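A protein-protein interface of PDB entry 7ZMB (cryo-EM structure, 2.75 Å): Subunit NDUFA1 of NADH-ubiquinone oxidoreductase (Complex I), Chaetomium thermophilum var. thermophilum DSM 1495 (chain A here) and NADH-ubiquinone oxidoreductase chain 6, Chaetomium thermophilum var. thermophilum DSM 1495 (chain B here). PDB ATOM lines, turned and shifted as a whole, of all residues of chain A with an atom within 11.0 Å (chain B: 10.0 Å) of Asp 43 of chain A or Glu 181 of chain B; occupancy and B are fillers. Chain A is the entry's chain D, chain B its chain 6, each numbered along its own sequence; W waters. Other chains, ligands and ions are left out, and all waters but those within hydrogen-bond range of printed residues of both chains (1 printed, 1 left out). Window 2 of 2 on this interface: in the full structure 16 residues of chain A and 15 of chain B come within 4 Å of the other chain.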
ATOM      1  N   ARG A  39      11.138 -11.493  -5.450  1.00  0.00           N
ATOM      2  CA  ARG A  39      11.785 -11.703  -4.138  1.00  0.00           C
ATOM      3  C   ARG A  39      12.919 -12.712  -4.271  1.00  0.00           C
ATOM      4  O   ARG A  39      12.794 -13.612  -5.085  1.00  0.00           O
ATOM      5  CB  ARG A  39      10.742 -12.250  -3.168  1.00  0.00           C
ATOM      6  CG  ARG A  39       9.538 -11.343  -2.973  1.00  0.00           C
ATOM      7  CD  ARG A  39       9.952 -10.064  -2.285  1.00  0.00           C
ATOM      8  NE  ARG A  39      10.554 -10.342  -0.993  1.00  0.00           N
ATOM      9  CZ  ARG A  39       9.868 -10.494   0.131  1.00  0.00           C
ATOM     10  NH1 ARG A  39       8.551 -10.402   0.114  1.00  0.00           N
ATOM     11  NH2 ARG A  39      10.498 -10.742   1.262  1.00  0.00           N
ATOM     12  N   TRP A  40      13.990 -12.552  -3.506  1.00  0.00           N
ATOM     13  CA  TRP A  40      15.117 -13.514  -3.483  1.00  0.00           C
ATOM     14  C   TRP A  40      15.540 -13.780  -2.041  1.00  0.00           C
ATOM     15  O   TRP A  40      15.135 -12.996  -1.170  1.00  0.00           O
ATOM     16  CB  TRP A  40      16.293 -13.007  -4.323  1.00  0.00           C
ATOM     17  CG  TRP A  40      16.894 -11.707  -3.892  1.00  0.00           C
ATOM     18  CD1 TRP A  40      17.950 -11.531  -3.049  1.00  0.00           C
ATOM     19  CD2 TRP A  40      16.499 -10.390  -4.317  1.00  0.00           C
ATOM     20  NE1 TRP A  40      18.229 -10.201  -2.906  1.00  0.00           N
ATOM     21  CE2 TRP A  40      17.354  -9.475  -3.670  1.00  0.00           C
ATOM     22  CE3 TRP A  40      15.501  -9.896  -5.163  1.00  0.00           C
ATOM     23  CZ2 TRP A  40      17.245  -8.097  -3.849  1.00  0.00           C
ATOM     24  CZ3 TRP A  40      15.396  -8.536  -5.342  1.00  0.00           C
ATOM     25  CH2 TRP A  40      16.258  -7.649  -4.694  1.00  0.00           C
ATOM     26  N   SER A  41      16.319 -14.843  -1.811  1.00  0.00           N
ATOM     27  CA  SER A  41      16.819 -15.195  -0.459  1.00  0.00           C
ATOM     28  C   SER A  41      15.633 -15.322   0.497  1.00  0.00           C
ATOM     29  O   SER A  41      15.673 -14.705   1.578  1.00  0.00           O
ATOM     30  CB  SER A  41      17.868 -14.234  -0.002  1.00  0.00           C
ATOM     31  OG  SER A  41      18.922 -14.181  -0.947  1.00  0.00           O
ATOM     32  N   VAL A  42      14.621 -16.087   0.107  1.00  0.00           N
ATOM     33  CA  VAL A  42      13.357 -16.171   0.895  1.00  0.00           C
ATOM     34  C   VAL A  42      13.438 -17.283   1.938  1.00  0.00           C
ATOM     35  O   VAL A  42      13.871 -18.389   1.588  1.00  0.00           O
ATOM     36  CB  VAL A  42      12.179 -16.406  -0.073  1.00  0.00           C
ATOM     37  CG1 VAL A  42      10.875 -16.691   0.647  1.00  0.00           C
ATOM     38  CG2 VAL A  42      12.013 -15.256  -1.055  1.00  0.00           C
ATOM     39  N   ASP A  43      13.043 -16.993   3.174  1.00  0.00           N
ATOM     40  CA  ASP A  43      13.005 -18.011   4.255  1.00  0.00           C
ATOM     41  C   ASP A  43      11.552 -18.370   4.578  1.00  0.00           C
ATOM     42  O   ASP A  43      10.658 -17.864   3.889  1.00  0.00           O
ATOM     43  CB  ASP A  43      13.826 -17.579   5.472  1.00  0.00           C
ATOM     44  CG  ASP A  43      13.438 -16.241   6.082  1.00  0.00           C
ATOM     45  OD1 ASP A  43      12.410 -15.680   5.675  1.00  0.00           O
ATOM     46  OD2 ASP A  43      14.174 -15.776   6.972  1.00  0.00           O
ATOM     47  N   GLN A  44      11.343 -19.228   5.575  1.00  0.00           N
ATOM     48  CA  GLN A  44       9.988 -19.661   5.979  1.00  0.00           C
ATOM     49  C   GLN A  44       9.142 -18.449   6.370  1.00  0.00           C
ATOM     50  O   GLN A  44       7.939 -18.487   6.112  1.00  0.00           O
ATOM     51  CB  GLN A  44      10.094 -20.702   7.093  1.00  0.00           C
ATOM     52  CG  GLN A  44       8.783 -21.407   7.414  1.00  0.00           C
ATOM     53  CD  GLN A  44       8.069 -21.950   6.198  1.00  0.00           C
ATOM     54  OE1 GLN A  44       6.848 -21.872   6.092  1.00  0.00           O
ATOM     55  NE2 GLN A  44       8.823 -22.508   5.264  1.00  0.00           N
ATOM     56  N   TRP A  45       9.762 -17.403   6.913  1.00  0.00           N
ATOM     57  CA  TRP A  45       9.029 -16.189   7.329  1.00  0.00           C
ATOM     58  C   TRP A  45       8.432 -15.544   6.081  1.00  0.00           C
ATOM     59  O   TRP A  45       7.227 -15.299   6.062  1.00  0.00           O
ATOM     60  CB  TRP A  45       9.968 -15.229   8.059  1.00  0.00           C
ATOM     61  CG  TRP A  45       9.312 -13.977   8.551  1.00  0.00           C
ATOM     62  CD1 TRP A  45       9.055 -12.845   7.836  1.00  0.00           C
ATOM     63  CD2 TRP A  45       8.845 -13.722   9.887  1.00  0.00           C
ATOM     64  NE1 TRP A  45       8.448 -11.911   8.628  1.00  0.00           N
ATOM     65  CE2 TRP A  45       8.309 -12.417   9.892  1.00  0.00           C
ATOM     66  CE3 TRP A  45       8.827 -14.463  11.072  1.00  0.00           C
ATOM     67  CZ2 TRP A  45       7.761 -11.844  11.037  1.00  0.00           C
ATOM     68  CZ3 TRP A  45       8.283 -13.896  12.203  1.00  0.00           C
ATOM     69  CH2 TRP A  45       7.755 -12.605  12.181  1.00  0.00           C
ATOM     70  N   ASP A  46       9.274 -15.288   5.076  1.00  0.00           N
ATOM     71  CA  ASP A  46       8.802 -14.591   3.848  1.00  0.00           C
ATOM     72  C   ASP A  46       7.774 -15.425   3.096  1.00  0.00           C
ATOM     73  O   ASP A  46       6.809 -14.845   2.594  1.00  0.00           O
ATOM     74  CB  ASP A  46       9.991 -14.211   2.968  1.00  0.00           C
ATOM     75  CG  ASP A  46      11.126 -13.545   3.721  1.00  0.00           C
ATOM     76  OD1 ASP A  46      10.837 -12.749   4.629  1.00  0.00           O
ATOM     77  OD2 ASP A  46      12.290 -13.841   3.402  1.00  0.00           O
ATOM     78  N   LYS A  47       8.025 -16.725   2.981  1.00  0.00           N
ATOM     79  CA  LYS A  47       7.078 -17.630   2.298  1.00  0.00           C
ATOM     80  C   LYS A  47       5.722 -17.541   2.997  1.00  0.00           C
ATOM     81  O   LYS A  47       4.714 -17.420   2.281  1.00  0.00           O
ATOM     82  CB  LYS A  47       7.621 -19.054   2.396  1.00  0.00           C
ATOM     83  CG  LYS A  47       8.664 -19.452   1.367  1.00  0.00           C
ATOM     84  CD  LYS A  47       9.226 -20.827   1.636  1.00  0.00           C
ATOM     85  CE  LYS A  47      10.533 -21.077   0.916  1.00  0.00           C
ATOM     86  NZ  LYS A  47      11.590 -20.144   1.369  1.00  0.00           N
ATOM     87  N   GLN A  48       5.710 -17.549   4.334  1.00  0.00           N
ATOM     88  CA  GLN A  48       4.455 -17.426   5.123  1.00  0.00           C
ATOM     89  C   GLN A  48       3.829 -16.044   4.925  1.00  0.00           C
ATOM     90  O   GLN A  48       2.609 -15.981   4.773  1.00  0.00           O
ATOM     91  CB  GLN A  48       4.746 -17.679   6.602  1.00  0.00           C
ATOM     92  CG  GLN A  48       4.974 -19.131   6.967  1.00  0.00           C
ATOM     93  CD  GLN A  48       5.241 -19.246   8.446  1.00  0.00           C
ATOM     94  OE1 GLN A  48       4.957 -18.331   9.214  1.00  0.00           O
ATOM     95  NE2 GLN A  48       5.771 -20.384   8.860  1.00  0.00           N
ATOM     96  N   GLN A  49       4.631 -14.981   4.952  1.00  0.00           N
ATOM     97  CA  GLN A  49       4.131 -13.590   4.765  1.00  0.00           C
ATOM     98  C   GLN A  49       3.534 -13.411   3.362  1.00  0.00           C
ATOM     99  O   GLN A  49       2.545 -12.678   3.251  1.00  0.00           O
ATOM    100  CB  GLN A  49       5.240 -12.571   5.044  1.00  0.00           C
ATOM    101  CG  GLN A  49       5.564 -12.382   6.519  1.00  0.00           C
ATOM    102  CD  GLN A  49       4.623 -11.446   7.238  1.00  0.00           C
ATOM    103  OE1 GLN A  49       3.619 -10.994   6.696  1.00  0.00           O
ATOM    104  NE2 GLN A  49       4.949 -11.142   8.481  1.00  0.00           N
ATOM    105  N   MET A  50       4.115 -14.043   2.335  1.00  0.00           N
ATOM    106  CA  MET A  50       3.574 -13.982   0.945  1.00  0.00           C
ATOM    107  C   MET A  50       2.218 -14.677   0.876  1.00  0.00           C
ATOM    108  O   MET A  50       1.357 -14.229   0.110  1.00  0.00           O
ATOM    109  CB  MET A  50       4.530 -14.565  -0.104  1.00  0.00           C
ATOM    110  CG  MET A  50       5.562 -13.558  -0.562  1.00  0.00           C
ATOM    111  SD  MET A  50       6.769 -14.198  -1.739  1.00  0.00           S
ATOM    112  CE  MET A  50       7.704 -15.302  -0.685  1.00  0.00           C
ATOM    113  N   GLU A  51       2.040 -15.724   1.673  1.00  0.00           N
ATOM    114  CA  GLU A  51       0.769 -16.477   1.632  1.00  0.00           C
ATOM    115  C   GLU A  51      -0.249 -15.654   2.410  1.00  0.00           C
ATOM    116  O   GLU A  51      -1.434 -15.716   2.060  1.00  0.00           O
ATOM    117  CB  GLU A  51       0.954 -17.840   2.284  1.00  0.00           C
ATOM    118  CG  GLU A  51       1.723 -18.828   1.435  1.00  0.00           C
ATOM    119  CD  GLU A  51       2.206 -20.027   2.233  1.00  0.00           C
ATOM    120  OE1 GLU A  51       2.424 -19.869   3.448  1.00  0.00           O
ATOM    121  OE2 GLU A  51       2.346 -21.113   1.640  1.00  0.00           O
ATOM    122  N   ARG A  52       0.227 -14.837   3.348  1.00  0.00           N
ATOM    123  CA  ARG A  52      -0.698 -13.997   4.141  1.00  0.00           C
ATOM    124  C   ARG A  52      -1.085 -12.774   3.301  1.00  0.00           C
ATOM    125  O   ARG A  52      -2.074 -12.129   3.644  1.00  0.00           O
ATOM    126  CB  ARG A  52      -0.118 -13.687   5.526  1.00  0.00           C
ATOM    127  CG  ARG A  52      -1.180 -13.301   6.545  1.00  0.00           C
ATOM    128  CD  ARG A  52      -0.646 -12.888   7.899  1.00  0.00           C
ATOM    129  NE  ARG A  52      -1.607 -12.025   8.569  1.00  0.00           N
ATOM    130  CZ  ARG A  52      -1.598 -10.701   8.502  1.00  0.00           C
ATOM    131  NH1 ARG A  52      -0.661 -10.079   7.807  1.00  0.00           N
ATOM    132  NH2 ARG A  52      -2.518 -10.000   9.138  1.00  0.00           N
ATOM    133  N   GLY B  65      13.299 -32.879   0.851  1.00  0.00           N
ATOM    134  CA  GLY B  65      13.796 -31.664   1.522  1.00  0.00           C
ATOM    135  C   GLY B  65      15.117 -31.825   2.247  1.00  0.00           C
ATOM    136  O   GLY B  65      15.561 -30.843   2.856  1.00  0.00           O
ATOM    137  N   ASN B  67      18.188 -31.529   1.403  1.00  0.00           N
ATOM    138  CA  ASN B  67      19.100 -31.062   0.325  1.00  0.00           C
ATOM    139  C   ASN B  67      20.585 -31.271   0.649  1.00  0.00           C
ATOM    140  O   ASN B  67      21.298 -31.708  -0.263  1.00  0.00           O
ATOM    141  CB  ASN B  67      18.792 -29.621  -0.095  1.00  0.00           C
ATOM    142  CG  ASN B  67      17.440 -29.479  -0.754  1.00  0.00           C
ATOM    143  OD1 ASN B  67      16.457 -29.154  -0.093  1.00  0.00           O
ATOM    144  ND2 ASN B  67      17.379 -29.726  -2.051  1.00  0.00           N
ATOM    145  N   ILE B 174       3.927 -21.321  11.989  1.00  0.00           N
ATOM    146  CA  ILE B 174       4.144 -20.642  13.300  1.00  0.00           C
ATOM    147  C   ILE B 174       5.050 -19.455  12.991  1.00  0.00           C
ATOM    148  O   ILE B 174       5.634 -19.442  11.905  1.00  0.00           O
ATOM    149  CB  ILE B 174       4.740 -21.534  14.413  1.00  0.00           C
ATOM    150  CG1 ILE B 174       6.020 -22.245  13.971  1.00  0.00           C
ATOM    151  CG2 ILE B 174       3.705 -22.499  14.970  1.00  0.00           C
ATOM    152  CD1 ILE B 174       6.734 -22.955  15.096  1.00  0.00           C
ATOM    153  N   TRP B 175       5.109 -18.479  13.886  1.00  0.00           N
ATOM    154  CA  TRP B 175       5.946 -17.275  13.684  1.00  0.00           C
ATOM    155  C   TRP B 175       7.110 -17.255  14.678  1.00  0.00           C
ATOM    156  O   TRP B 175       8.192 -16.799  14.298  1.00  0.00           O
ATOM    157  CB  TRP B 175       5.037 -16.052  13.803  1.00  0.00           C
ATOM    158  CG  TRP B 175       3.976 -16.045  12.746  1.00  0.00           C
ATOM    159  CD1 TRP B 175       2.684 -16.459  12.873  1.00  0.00           C
ATOM    160  CD2 TRP B 175       4.129 -15.630  11.376  1.00  0.00           C
ATOM    161  NE1 TRP B 175       2.019 -16.315  11.688  1.00  0.00           N
ATOM    162  CE2 TRP B 175       2.878 -15.809  10.749  1.00  0.00           C
ATOM    163  CE3 TRP B 175       5.189 -15.115  10.624  1.00  0.00           C
ATOM    164  CZ2 TRP B 175       2.663 -15.493   9.410  1.00  0.00           C
ATOM    165  CZ3 TRP B 175       4.978 -14.806   9.300  1.00  0.00           C
ATOM    166  CH2 TRP B 175       3.730 -14.988   8.705  1.00  0.00           C
ATOM    167  N   ASP B 176       6.896 -17.759  15.889  1.00  0.00           N
ATOM    168  CA  ASP B 176       7.945 -17.778  16.945  1.00  0.00           C
ATOM    169  C   ASP B 176       9.080 -18.715  16.521  1.00  0.00           C
ATOM    170  O   ASP B 176      10.236 -18.407  16.816  1.00  0.00           O
ATOM    171  CB  ASP B 176       7.370 -18.110  18.321  1.00  0.00           C
ATOM    172  CG  ASP B 176       6.145 -17.302  18.704  1.00  0.00           C
ATOM    173  OD1 ASP B 176       5.586 -16.629  17.826  1.00  0.00           O
ATOM    174  OD2 ASP B 176       5.759 -17.355  19.883  1.00  0.00           O
ATOM    175  N   GLY B 177       8.746 -19.819  15.860  1.00  0.00           N
ATOM    176  CA  GLY B 177       9.756 -20.778  15.380  1.00  0.00           C
ATOM    177  C   GLY B 177      10.258 -20.431  13.997  1.00  0.00           C
ATOM    178  O   GLY B 177      11.041 -21.209  13.455  1.00  0.00           O
ATOM    179  N   ALA B 178       9.799 -19.311  13.444  1.00  0.00           N
ATOM    180  CA  ALA B 178      10.252 -18.871  12.107  1.00  0.00           C
ATOM    181  C   ALA B 178      11.073 -17.584  12.178  1.00  0.00           C
ATOM    182  O   ALA B 178      11.352 -17.031  11.099  1.00  0.00           O
ATOM    183  CB  ALA B 178       9.069 -18.685  11.204  1.00  0.00           C
ATOM    184  N   LEU B 179      11.448 -17.115  13.371  1.00  0.00           N
ATOM    185  CA  LEU B 179      12.146 -15.809  13.411  1.00  0.00           C
ATOM    186  C   LEU B 179      13.441 -15.871  12.593  1.00  0.00           C
ATOM    187  O   LEU B 179      13.666 -14.958  11.795  1.00  0.00           O
ATOM    188  CB  LEU B 179      12.434 -15.444  14.870  1.00  0.00           C
ATOM    189  CG  LEU B 179      13.353 -14.240  15.067  1.00  0.00           C
ATOM    190  CD1 LEU B 179      12.667 -12.956  14.639  1.00  0.00           C
ATOM    191  CD2 LEU B 179      13.807 -14.137  16.507  1.00  0.00           C
ATOM    192  N   ALA B 180      14.270 -16.893  12.787  1.00  0.00           N
ATOM    193  CA  ALA B 180      15.467 -17.076  11.937  1.00  0.00           C
ATOM    194  C   ALA B 180      15.573 -18.534  11.481  1.00  0.00           C
ATOM    195  O   ALA B 180      16.425 -19.231  12.025  1.00  0.00           O
ATOM    196  CB  ALA B 180      16.693 -16.656  12.688  1.00  0.00           C
ATOM    197  N   GLU B 181      14.754 -18.948  10.480  1.00  0.00           N
ATOM    198  CA  GLU B 181      14.801 -20.375  10.063  1.00  0.00           C
ATOM    199  C   GLU B 181      16.188 -20.679   9.494  1.00  0.00           C
ATOM    200  O   GLU B 181      16.640 -19.929   8.613  1.00  0.00           O
ATOM    201  CB  GLU B 181      13.693 -20.716   9.070  1.00  0.00           C
ATOM    202  CG  GLU B 181      13.855 -22.068   8.400  1.00  0.00           C
ATOM    203  CD  GLU B 181      14.073 -21.998   6.899  1.00  0.00           C
ATOM    204  OE1 GLU B 181      13.764 -20.947   6.307  1.00  0.00           O
ATOM    205  OE2 GLU B 181      14.563 -22.990   6.326  1.00  0.00           O
ATOM    206  N   ASN B 182      16.844 -21.754  10.034  1.00  0.00           N
ATOM    207  CA  ASN B 182      18.190 -22.108   9.522  1.00  0.00           C
ATOM    208  C   ASN B 182      18.061 -23.156   8.421  1.00  0.00           C
ATOM    209  O   ASN B 182      16.994 -23.769   8.335  1.00  0.00           O
ATOM    210  CB  ASN B 182      19.096 -22.672  10.621  1.00  0.00           C
ATOM    211  CG  ASN B 182      19.526 -21.672  11.669  1.00  0.00           C
ATOM    212  OD1 ASN B 182      18.719 -20.902  12.173  1.00  0.00           O
ATOM    213  ND2 ASN B 182      20.795 -21.708  12.030  1.00  0.00           N
ATOM    214  N   ASN B 183      19.103 -23.348   7.616  1.00  0.00           N
ATOM    215  CA  ASN B 183      19.090 -24.472   6.646  1.00  0.00           C
ATOM    216  C   ASN B 183      19.621 -25.698   7.375  1.00  0.00           C
ATOM    217  O   ASN B 183      20.328 -25.515   8.359  1.00  0.00           O
ATOM    218  CB  ASN B 183      19.899 -24.138   5.390  1.00  0.00           C
ATOM    219  CG  ASN B 183      19.504 -22.821   4.765  1.00  0.00           C
ATOM    220  OD1 ASN B 183      18.323 -22.553   4.567  1.00  0.00           O
ATOM    221  ND2 ASN B 183      20.485 -21.994   4.443  1.00  0.00           N
ATOM    222  N   HIS B 184      19.216 -26.887   6.989  1.00  0.00           N
ATOM    223  CA  HIS B 184      19.619 -28.087   7.750  1.00  0.00           C
ATOM    224  C   HIS B 184      21.145 -28.170   7.884  1.00  0.00           C
ATOM    225  O   HIS B 184      21.591 -28.678   8.912  1.00  0.00           O
ATOM    226  CB  HIS B 184      19.066 -29.326   7.036  1.00  0.00           C
ATOM    227  CG  HIS B 184      17.583 -29.408   6.930  1.00  0.00           C
ATOM    228  ND1 HIS B 184      16.957 -30.464   6.301  1.00  0.00           N
ATOM    229  CD2 HIS B 184      16.604 -28.590   7.362  1.00  0.00           C
ATOM    230  CE1 HIS B 184      15.657 -30.292   6.350  1.00  0.00           C
ATOM    231  NE2 HIS B 184      15.415 -29.148   6.988  1.00  0.00           N
ATOM    232  N   ILE B 185      21.913 -27.709   6.899  1.00  0.00           N
ATOM    233  CA  ILE B 185      23.406 -27.700   7.005  1.00  0.00           C
ATOM    234  C   ILE B 185      23.827 -26.785   8.157  1.00  0.00           C
ATOM    235  O   ILE B 185      24.797 -27.131   8.845  1.00  0.00           O
ATOM    236  CB  ILE B 185      24.105 -27.371   5.671  1.00  0.00           C
ATOM    237  CG1 ILE B 185      25.626 -27.403   5.834  1.00  0.00           C
ATOM    238  CG2 ILE B 185      23.614 -26.050   5.098  1.00  0.00           C
ATOM    239  CD1 ILE B 185      26.396 -27.015   4.602  1.00  0.00           C
ATOM    240  N   SER B 186      23.121 -25.669   8.361  1.00  0.00           N
ATOM    241  CA  SER B 186      23.420 -24.763   9.495  1.00  0.00           C
ATOM    242  C   SER B 186      22.921 -25.365  10.819  1.00  0.00           C
ATOM    243  O   SER B 186      23.613 -25.198  11.822  1.00  0.00           O
ATOM    244  CB  SER B 186      22.871 -23.388   9.224  1.00  0.00           C
ATOM    245  OG  SER B 186      23.262 -22.483  10.243  1.00  0.00           O
ATOM    246  N   SER B 187      21.792 -26.068  10.811  1.00  0.00           N
ATOM    247  CA  SER B 187      21.230 -26.695  12.033  1.00  0.00           C
ATOM    248  C   SER B 187      22.197 -27.747  12.557  1.00  0.00           C
ATOM    249  O   SER B 187      22.319 -27.889  13.783  1.00  0.00           O
ATOM    250  CB  SER B 187      19.882 -27.272  11.797  1.00  0.00           C
ATOM    251  OG  SER B 187      19.076 -26.360  11.076  1.00  0.00           O
ATOM    252  N   ASN B 190      25.228 -25.916  13.904  1.00  0.00           N
ATOM    253  CA  ASN B 190      24.958 -25.310  15.201  1.00  0.00           C
ATOM    254  C   ASN B 190      25.342 -26.219  16.358  1.00  0.00           C
ATOM    255  O   ASN B 190      25.504 -25.735  17.480  1.00  0.00           O
ATOM    256  CB  ASN B 190      23.482 -24.934  15.309  1.00  0.00           C
ATOM    257  CG  ASN B 190      23.139 -23.667  14.548  1.00  0.00           C
ATOM    258  OD1 ASN B 190      24.013 -22.882  14.194  1.00  0.00           O
ATOM    259  ND2 ASN B 190      21.854 -23.468  14.290  1.00  0.00           N
HETATM  260  O   HOH W   1      16.965 -16.939   8.383  1.00  0.00           O
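Among the printed residues, pairs that only touch across the chains: Asp 43 of chain A with Glu 181 of chain B, Trp 45 of chain A with Trp 175 of chain B, Trp 45 of chain A with Ala 178 of chain B, Gln 48 of chain A with Trp 175 of chain B and Gln 49 of chain A with Trp 175 of chain B.
Of chain B, only Glu 181 comes within 4 Å of Asp 43 of chain A. Of the printed residues of chain A, Glu 181 of chain B touches Asp 43 (3.5 Å) and Gln 44 (3.1 Å). Val 42 of chain A touches none of the printed residues of chain B. Of the printed residues of chain A, Ala 178 of chain B touches Trp 45. No residue of chain A comes within 4 Å of Asn 182 of chain B. No residue of chain A comes within 4 Å of Asn 183 of chain B. Printed residues of chain A within 4 Å of Ile 174 of chain B: Gln 48. Of the printed residues of chain A, Trp 175 of chain B touches Trp 45 (3.6 Å), Gln 48 (3.5 Å) and Gln 49 (3.7 Å). Of the printed residues of chain B, Gln 44 of chain A touches Glu 181 (3.1 Å). Asn 67 of chain B touches none of the printed residues of chain A. The nearest residue of chain B that does not touch Asp 43 of chain A is Leu 179 of chain B (4.9 Å). The nearest printed residue of chain A that does not touch Glu 181 of chain B is Val 42 of chain A (5.4 Å). The nearest printed residue of chain A that does not touch Trp 175 of chain B is Arg 52 of chain A (4.5 Å).
Water W1 lies within hydrogen-bond range of the backbone carbonyl oxygen (O) of Glu 181 of chain B and the side-chain carboxylate (OD2) of Asp 43 of chain A.
N of Gln 44 of chain A sits at hydrogen-bond distance from OE1 of Glu 181 of chain B, at 3.1 Å. The side-chain amide oxygen (OE1) of Gln 48 of chain A sits close to the backbone carbonyl oxygen (O) of Ile 174 of chain B (3.0 Å).
Of the 17 printed residues of chain B, 4 touch a printed residue of chain A. Printed residues of chain B that touch a printed residue of chain A: Ile 174, Trp 175, Ala 178 and Glu 181. Hydrophobic or aromatic side chains of chain A that line the printed part of chain B: Trp 45. Among the printed residues, 7 pairs touch across the chains.
The side-chain amide nitrogen (NE2) of Gln 48 of chain A is in hydrogen-bond range of the side-chain amide oxygen (OE1) of Gln 44 of chain A (3.3 Å). The side-chain carboxylate of Asp 43 of chain A sits close to the backbone NH of Trp 45 of chain A (3.4 Å). OD1 of Asp 43 of chain A sits close to N of Asp 46 of chain A, at 3.2 Å.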
